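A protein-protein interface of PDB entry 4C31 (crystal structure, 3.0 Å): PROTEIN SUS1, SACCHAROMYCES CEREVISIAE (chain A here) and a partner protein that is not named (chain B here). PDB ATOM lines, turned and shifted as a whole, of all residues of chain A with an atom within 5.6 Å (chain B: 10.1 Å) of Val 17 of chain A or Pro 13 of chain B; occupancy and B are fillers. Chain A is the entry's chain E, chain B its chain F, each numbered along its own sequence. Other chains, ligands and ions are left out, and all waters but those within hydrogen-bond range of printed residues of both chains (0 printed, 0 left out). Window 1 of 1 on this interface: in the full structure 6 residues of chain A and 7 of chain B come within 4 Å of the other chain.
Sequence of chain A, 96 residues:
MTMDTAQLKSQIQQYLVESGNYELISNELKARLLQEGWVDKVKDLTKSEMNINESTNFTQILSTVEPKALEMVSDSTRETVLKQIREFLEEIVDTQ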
ATOM      1  N   ILE A  12      -7.425  14.899  -4.983  1.00  0.00           N
ATOM      2  CA  ILE A  12      -8.606  14.795  -5.839  1.00  0.00           C
ATOM      3  C   ILE A  12      -9.002  13.333  -6.031  1.00  0.00           C
ATOM      4  O   ILE A  12     -10.132  12.941  -5.730  1.00  0.00           O
ATOM      5  CB  ILE A  12      -8.362  15.444  -7.219  1.00  0.00           C
ATOM      6  CG1 ILE A  12      -8.194  16.955  -7.068  1.00  0.00           C
ATOM      7  CG2 ILE A  12      -9.519  15.150  -8.174  1.00  0.00           C
ATOM      8  CD1 ILE A  12      -7.759  17.667  -8.340  1.00  0.00           C
ATOM      9  N   GLN A  13      -8.067  12.537  -6.540  1.00  0.00           N
ATOM     10  CA  GLN A  13      -8.319  11.124  -6.800  1.00  0.00           C
ATOM     11  C   GLN A  13      -8.726  10.401  -5.528  1.00  0.00           C
ATOM     12  O   GLN A  13      -9.561   9.497  -5.559  1.00  0.00           O
ATOM     13  CB  GLN A  13      -7.088  10.452  -7.404  1.00  0.00           C
ATOM     14  CG  GLN A  13      -7.376   9.073  -7.974  1.00  0.00           C
ATOM     15  CD  GLN A  13      -6.126   8.357  -8.433  1.00  0.00           C
ATOM     16  OE1 GLN A  13      -5.721   8.464  -9.593  1.00  0.00           O
ATOM     17  NE2 GLN A  13      -5.502   7.622  -7.520  1.00  0.00           N
ATOM     18  N   GLN A  14      -8.127  10.795  -4.410  1.00  0.00           N
ATOM     19  CA  GLN A  14      -8.440  10.182  -3.128  1.00  0.00           C
ATOM     20  C   GLN A  14      -9.919  10.367  -2.841  1.00  0.00           C
ATOM     21  O   GLN A  14     -10.656   9.401  -2.637  1.00  0.00           O
ATOM     22  CB  GLN A  14      -7.586  10.792  -2.011  1.00  0.00           C
ATOM     23  CG  GLN A  14      -7.855  10.221  -0.621  1.00  0.00           C
ATOM     24  CD  GLN A  14      -7.261  11.063   0.504  1.00  0.00           C
ATOM     25  OE1 GLN A  14      -7.655  10.922   1.660  1.00  0.00           O
ATOM     26  NE2 GLN A  14      -6.304  11.931   0.174  1.00  0.00           N
ATOM     27  N   TYR A  15     -10.343  11.626  -2.858  1.00  0.00           N
ATOM     28  CA  TYR A  15     -11.712  11.982  -2.525  1.00  0.00           C
ATOM     29  C   TYR A  15     -12.661  11.563  -3.639  1.00  0.00           C
ATOM     30  O   TYR A  15     -13.828  11.271  -3.385  1.00  0.00           O
ATOM     31  CB  TYR A  15     -11.812  13.485  -2.257  1.00  0.00           C
ATOM     32  CG  TYR A  15     -11.060  13.926  -1.015  1.00  0.00           C
ATOM     33  CD1 TYR A  15     -11.211  13.249   0.190  1.00  0.00           C
ATOM     34  CD2 TYR A  15     -10.191  15.010  -1.051  1.00  0.00           C
ATOM     35  CE1 TYR A  15     -10.526  13.644   1.327  1.00  0.00           C
ATOM     36  CE2 TYR A  15      -9.499  15.410   0.081  1.00  0.00           C
ATOM     37  CZ  TYR A  15      -9.672  14.725   1.265  1.00  0.00           C
ATOM     38  OH  TYR A  15      -8.988  15.121   2.393  1.00  0.00           O
ATOM     39  N   LEU A  16     -12.154  11.526  -4.869  1.00  0.00           N
ATOM     40  CA  LEU A  16     -12.944  11.061  -6.005  1.00  0.00           C
ATOM     41  C   LEU A  16     -13.390   9.619  -5.798  1.00  0.00           C
ATOM     42  O   LEU A  16     -14.523   9.256  -6.112  1.00  0.00           O
ATOM     43  CB  LEU A  16     -12.143  11.171  -7.303  1.00  0.00           C
ATOM     44  CG  LEU A  16     -12.801  10.547  -8.541  1.00  0.00           C
ATOM     45  CD1 LEU A  16     -14.034  11.330  -8.953  1.00  0.00           C
ATOM     46  CD2 LEU A  16     -11.812  10.448  -9.691  1.00  0.00           C
ATOM     47  N   VAL A  17     -12.486   8.798  -5.272  1.00  0.00           N
ATOM     48  CA  VAL A  17     -12.764   7.384  -5.064  1.00  0.00           C
ATOM     49  C   VAL A  17     -13.550   7.151  -3.782  1.00  0.00           C
ATOM     50  O   VAL A  17     -14.515   6.391  -3.772  1.00  0.00           O
ATOM     51  CB  VAL A  17     -11.465   6.565  -5.007  1.00  0.00           C
ATOM     52  CG1 VAL A  17     -11.758   5.115  -4.642  1.00  0.00           C
ATOM     53  CG2 VAL A  17     -10.732   6.638  -6.343  1.00  0.00           C
ATOM     54  N   GLU A  18     -13.127   7.805  -2.705  1.00  0.00           N
ATOM     55  CA  GLU A  18     -13.736   7.599  -1.395  1.00  0.00           C
ATOM     56  C   GLU A  18     -15.172   8.103  -1.349  1.00  0.00           C
ATOM     57  O   GLU A  18     -16.024   7.516  -0.678  1.00  0.00           O
ATOM     58  CB  GLU A  18     -12.911   8.292  -0.306  1.00  0.00           C
ATOM     59  CG  GLU A  18     -11.556   7.644  -0.059  1.00  0.00           C
ATOM     60  CD  GLU A  18     -10.668   8.454   0.867  1.00  0.00           C
ATOM     61  OE1 GLU A  18     -11.176   9.385   1.528  1.00  0.00           O
ATOM     62  OE2 GLU A  18      -9.458   8.150   0.934  1.00  0.00           O
ATOM     63  N   SER A  19     -15.436   9.191  -2.067  1.00  0.00           N
ATOM     64  CA  SER A  19     -16.764   9.797  -2.084  1.00  0.00           C
ATOM     65  C   SER A  19     -17.756   8.988  -2.918  1.00  0.00           C
ATOM     66  O   SER A  19     -18.967   9.184  -2.816  1.00  0.00           O
ATOM     67  CB  SER A  19     -16.683  11.223  -2.623  1.00  0.00           C
ATOM     68  OG  SER A  19     -16.105  11.239  -3.917  1.00  0.00           O
ATOM     69  N   GLY A  20     -17.234   8.083  -3.742  1.00  0.00           N
ATOM     70  CA  GLY A  20     -18.063   7.214  -4.558  1.00  0.00           C
ATOM     71  C   GLY A  20     -18.270   7.739  -5.966  1.00  0.00           C
ATOM     72  O   GLY A  20     -18.934   7.110  -6.788  1.00  0.00           O
ATOM     73  N   ASN A  21     -17.707   8.903  -6.253  1.00  0.00           N
ATOM     74  CA  ASN A  21     -17.902   9.503  -7.559  1.00  0.00           C
ATOM     75  C   ASN A  21     -17.176   8.732  -8.661  1.00  0.00           C
ATOM     76  O   ASN A  21     -17.664   8.671  -9.791  1.00  0.00           O
ATOM     77  CB  ASN A  21     -17.457  10.962  -7.531  1.00  0.00           C
ATOM     78  CG  ASN A  21     -18.434  11.846  -6.778  1.00  0.00           C
ATOM     79  OD1 ASN A  21     -19.235  12.558  -7.382  1.00  0.00           O
ATOM     80  ND2 ASN A  21     -18.386  11.787  -5.450  1.00  0.00           N
ATOM     81  N   TYR A  22     -16.041   8.113  -8.339  1.00  0.00           N
ATOM     82  CA  TYR A  22     -15.338   7.308  -9.336  1.00  0.00           C
ATOM     83  C   TYR A  22     -16.196   6.131  -9.784  1.00  0.00           C
ATOM     84  O   TYR A  22     -16.282   5.827 -10.977  1.00  0.00           O
ATOM     85  CB  TYR A  22     -14.002   6.766  -8.822  1.00  0.00           C
ATOM     86  CG  TYR A  22     -13.509   5.678  -9.744  1.00  0.00           C
ATOM     87  CD1 TYR A  22     -12.923   5.996 -10.961  1.00  0.00           C
ATOM     88  CD2 TYR A  22     -13.683   4.336  -9.433  1.00  0.00           C
ATOM     89  CE1 TYR A  22     -12.504   5.016 -11.829  1.00  0.00           C
ATOM     90  CE2 TYR A  22     -13.268   3.349 -10.300  1.00  0.00           C
ATOM     91  CZ  TYR A  22     -12.680   3.698 -11.498  1.00  0.00           C
ATOM     92  OH  TYR A  22     -12.254   2.733 -12.373  1.00  0.00           O
ATOM     93  N   SER B   9     -17.306  -2.861   0.142  1.00  0.00           N
ATOM     94  CA  SER B   9     -16.015  -2.182   0.133  1.00  0.00           C
ATOM     95  C   SER B   9     -16.004  -1.122  -0.958  1.00  0.00           C
ATOM     96  O   SER B   9     -16.914  -1.071  -1.790  1.00  0.00           O
ATOM     97  CB  SER B   9     -14.875  -3.183  -0.080  1.00  0.00           C
ATOM     98  OG  SER B   9     -13.616  -2.530  -0.116  1.00  0.00           O
ATOM     99  N   ILE B  10     -14.981  -0.271  -0.949  1.00  0.00           N
ATOM    100  CA  ILE B  10     -14.906   0.821  -1.911  1.00  0.00           C
ATOM    101  C   ILE B  10     -14.266   0.354  -3.217  1.00  0.00           C
ATOM    102  O   ILE B  10     -13.325  -0.453  -3.231  1.00  0.00           O
ATOM    103  CB  ILE B  10     -14.129   2.031  -1.334  1.00  0.00           C
ATOM    104  CG1 ILE B  10     -14.954   2.692  -0.226  1.00  0.00           C
ATOM    105  CG2 ILE B  10     -13.813   3.056  -2.431  1.00  0.00           C
ATOM    106  CD1 ILE B  10     -14.296   3.898   0.428  1.00  0.00           C
ATOM    107  N   VAL B  11     -14.809   0.886  -4.306  1.00  0.00           N
ATOM    108  CA  VAL B  11     -14.383   0.575  -5.663  1.00  0.00           C
ATOM    109  C   VAL B  11     -13.094   1.307  -6.009  1.00  0.00           C
ATOM    110  O   VAL B  11     -13.089   2.532  -6.086  1.00  0.00           O
ATOM    111  CB  VAL B  11     -15.491   0.974  -6.677  1.00  0.00           C
ATOM    112  CG1 VAL B  11     -15.019   0.809  -8.124  1.00  0.00           C
ATOM    113  CG2 VAL B  11     -16.760   0.163  -6.425  1.00  0.00           C
ATOM    114  N   LEU B  12     -12.009   0.572  -6.231  1.00  0.00           N
ATOM    115  CA  LEU B  12     -10.758   1.207  -6.649  1.00  0.00           C
ATOM    116  C   LEU B  12     -10.616   1.215  -8.170  1.00  0.00           C
ATOM    117  O   LEU B  12     -11.030   0.271  -8.838  1.00  0.00           O
ATOM    118  CB  LEU B  12      -9.557   0.507  -6.019  1.00  0.00           C
ATOM    119  CG  LEU B  12      -9.142   1.108  -4.676  1.00  0.00           C
ATOM    120  CD1 LEU B  12     -10.174   0.812  -3.586  1.00  0.00           C
ATOM    121  CD2 LEU B  12      -7.783   0.582  -4.294  1.00  0.00           C
ATOM    122  N   PRO B  13     -10.062   2.302  -8.728  1.00  0.00           N
ATOM    123  CA  PRO B  13      -9.804   2.300 -10.174  1.00  0.00           C
ATOM    124  C   PRO B  13      -8.724   1.303 -10.576  1.00  0.00           C
ATOM    125  O   PRO B  13      -7.853   0.969  -9.768  1.00  0.00           O
ATOM    126  CB  PRO B  13      -9.350   3.735 -10.466  1.00  0.00           C
ATOM    127  CG  PRO B  13      -9.005   4.332  -9.146  1.00  0.00           C
ATOM    128  CD  PRO B  13      -9.793   3.612  -8.110  1.00  0.00           C
ATOM    129  N   THR B  14      -8.784   0.835 -11.817  1.00  0.00           N
ATOM    130  CA  THR B  14      -7.771  -0.077 -12.327  1.00  0.00           C
ATOM    131  C   THR B  14      -6.507   0.682 -12.704  1.00  0.00           C
ATOM    132  O   THR B  14      -6.456   1.911 -12.647  1.00  0.00           O
ATOM    133  CB  THR B  14      -8.260  -0.859 -13.558  1.00  0.00           C
ATOM    134  OG1 THR B  14      -8.286   0.008 -14.698  1.00  0.00           O
ATOM    135  CG2 THR B  14      -9.646  -1.437 -13.317  1.00  0.00           C
ATOM    136  N   VAL B  15      -5.479  -0.070 -13.078  1.00  0.00           N
ATOM    137  CA  VAL B  15      -4.211   0.504 -13.497  1.00  0.00           C
ATOM    138  C   VAL B  15      -4.411   1.414 -14.719  1.00  0.00           C
ATOM    139  O   VAL B  15      -3.615   2.321 -14.964  1.00  0.00           O
ATOM    140  CB  VAL B  15      -3.184  -0.619 -13.805  1.00  0.00           C
ATOM    141  CG1 VAL B  15      -3.653  -1.478 -14.980  1.00  0.00           C
ATOM    142  CG2 VAL B  15      -1.790  -0.045 -14.055  1.00  0.00           C
ATOM    143  N   GLY B  16      -5.487   1.180 -15.467  1.00  0.00           N
ATOM    144  CA  GLY B  16      -5.770   1.954 -16.663  1.00  0.00           C
ATOM    145  C   GLY B  16      -6.173   3.397 -16.398  1.00  0.00           C
ATOM    146  O   GLY B  16      -6.018   4.255 -17.265  1.00  0.00           O
ATOM    147  N   PHE B  17      -6.669   3.672 -15.196  1.00  0.00           N
ATOM    148  CA  PHE B  17      -7.098   5.019 -14.833  1.00  0.00           C
ATOM    149  C   PHE B  17      -5.890   5.875 -14.485  1.00  0.00           C
ATOM    150  O   PHE B  17      -5.515   5.988 -13.319  1.00  0.00           O
ATOM    151  CB  PHE B  17      -8.073   4.958 -13.656  1.00  0.00           C
ATOM    152  CG  PHE B  17      -8.713   6.273 -13.324  1.00  0.00           C
ATOM    153  CD1 PHE B  17      -9.800   6.726 -14.046  1.00  0.00           C
ATOM    154  CD2 PHE B  17      -8.238   7.045 -12.280  1.00  0.00           C
ATOM    155  CE1 PHE B  17     -10.397   7.933 -13.742  1.00  0.00           C
ATOM    156  CE2 PHE B  17      -8.827   8.251 -11.971  1.00  0.00           C
ATOM    157  CZ  PHE B  17      -9.911   8.698 -12.702  1.00  0.00           C
ATOM    158  N   ASP B  18      -5.298   6.497 -15.500  1.00  0.00           N
ATOM    159  CA  ASP B  18      -4.007   7.164 -15.341  1.00  0.00           C
ATOM    160  C   ASP B  18      -4.128   8.661 -15.083  1.00  0.00           C
ATOM    161  O   ASP B  18      -3.578   9.475 -15.821  1.00  0.00           O
ATOM    162  CB  ASP B  18      -3.139   6.922 -16.578  1.00  0.00           C
ATOM    163  CG  ASP B  18      -3.783   7.424 -17.854  1.00  0.00           C
ATOM    164  OD1 ASP B  18      -5.016   7.614 -17.865  1.00  0.00           O
ATOM    165  OD2 ASP B  18      -3.055   7.633 -18.845  1.00  0.00           O
ATOM    166  N   PHE B  19      -4.816   9.020 -14.007  1.00  0.00           N
ATOM    167  CA  PHE B  19      -4.962  10.420 -13.644  1.00  0.00           C
ATOM    168  C   PHE B  19      -3.591  11.038 -13.364  1.00  0.00           C
ATOM    169  O   PHE B  19      -3.255  12.075 -13.932  1.00  0.00           O
ATOM    170  CB  PHE B  19      -5.895  10.556 -12.435  1.00  0.00           C
ATOM    171  CG  PHE B  19      -6.123  11.975 -11.994  1.00  0.00           C
ATOM    172  CD1 PHE B  19      -6.251  12.994 -12.924  1.00  0.00           C
ATOM    173  CD2 PHE B  19      -6.235  12.285 -10.646  1.00  0.00           C
ATOM    174  CE1 PHE B  19      -6.461  14.298 -12.521  1.00  0.00           C
ATOM    175  CE2 PHE B  19      -6.450  13.586 -10.236  1.00  0.00           C
ATOM    176  CZ  PHE B  19      -6.564  14.594 -11.175  1.00  0.00           C
ATOM    177  N   ILE B  20      -2.783  10.385 -12.532  1.00  0.00           N
ATOM    178  CA  ILE B  20      -1.432  10.875 -12.254  1.00  0.00           C
ATOM    179  C   ILE B  20      -0.444  10.203 -13.203  1.00  0.00           C
ATOM    180  O   ILE B  20      -0.312   8.978 -13.210  1.00  0.00           O
ATOM    181  CB  ILE B  20      -0.994  10.615 -10.798  1.00  0.00           C
ATOM    182  CG1 ILE B  20      -2.134  10.913  -9.823  1.00  0.00           C
ATOM    183  CG2 ILE B  20       0.211  11.477 -10.454  1.00  0.00           C
ATOM    184  CD1 ILE B  20      -2.824   9.681  -9.313  1.00  0.00           C
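O of Leu 16 of chain A lies within hydrogen-bond range of N of Tyr 22 of chain A (2.9 Å).
The side-chain hydroxyl (OG1) of Thr 14 of chain B sits close to the backbone NH (N) of Gly 16 of chain B (3.1 Å).
O of Leu 16 of chain A sits at hydrogen-bond distance from OG of Ser 19 of chain A, 3.4 Å away.
The backbone carbonyl oxygen of Leu 16 of chain A sits at hydrogen-bond distance from the backbone NH of Asn 21 of chain A (3.2 Å).
OE1 of Gln 13 of chain A touches CE2 of Phe 17 of chain B (3.9 Å).
OE1 of Gln 13 of chain A touches CB of Phe 19 of chain B, 3.5 Å away.
Ile 20 of chain B touches Gln 13 of chain A (CD1 to OE1, 3.2 Å).
Leu 16 of chain A touches Phe 17 of chain B (CD2 to CZ, 3.97 Å).
Val 17 of chain A touches Val 11 of chain B (CG1 to O, 3.2 Å).
Val 17 of chain A touches Pro 13 of chain B (CG2 to CD, 3.6 Å).
Tyr 22 of chain A touches Val 11 of chain B.
Pro 13 of chain B touches Tyr 22 of chain A.
Tyr 22 of chain A touches Thr 14 of chain B (OH to N, 3.99 Å).
Tyr 22 of chain A touches Phe 17 of chain B (CE1 to CD1, 3.9 Å).
Leu 16 of chain A touches just one residue of chain B: Phe 17 (3.97 Å).
Of the printed residues of chain B, Val 17 of chain A touches Ile 10 (3.7 Å), Val 11 (3.2 Å) and Pro 13 (3.6 Å).
Glu 18 of chain A touches none of the printed residues of chain B.
No residue of chain B comes within 4 Å of Gly 20 of chain A.
Of the printed residues of chain A, Ile 10 of chain B touches Val 17.
Printed residues of chain A within 4 Å of Val 11 of chain B: Val 17 and Tyr 22.
Pro 13 of chain B touches just these residues of chain A: Val 17 (3.6 Å) and Tyr 22 (3.3 Å).
Of the printed residues of chain A, Phe 19 of chain B touches Gln 13 (3.5 Å).
Of the printed residues of chain A, Ile 20 of chain B touches Gln 13.
The nearest residue of chain B that does not touch Val 17 of chain A is Leu 12 of chain B (4.5 Å).
Hydrophobic or aromatic side chains of chain A that line the printed part of chain B: Leu 16, Val 17 and Tyr 22.
Printed residues of chain B that touch a printed residue of chain A: Ile 10, Val 11, Pro 13, Thr 14, Phe 17, Phe 19 and Ile 20.
Hydrophobic or aromatic side chains of chain B within 4 Å of the printed part of chain A: Ile 10, Val 11, Pro 13, Phe 17, Phe 19 and Ile 20.
Among the printed residues, no Asp or Glu carboxylate lies within 4 Å of a Lys or Arg side-chain nitrogen of the other chain.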
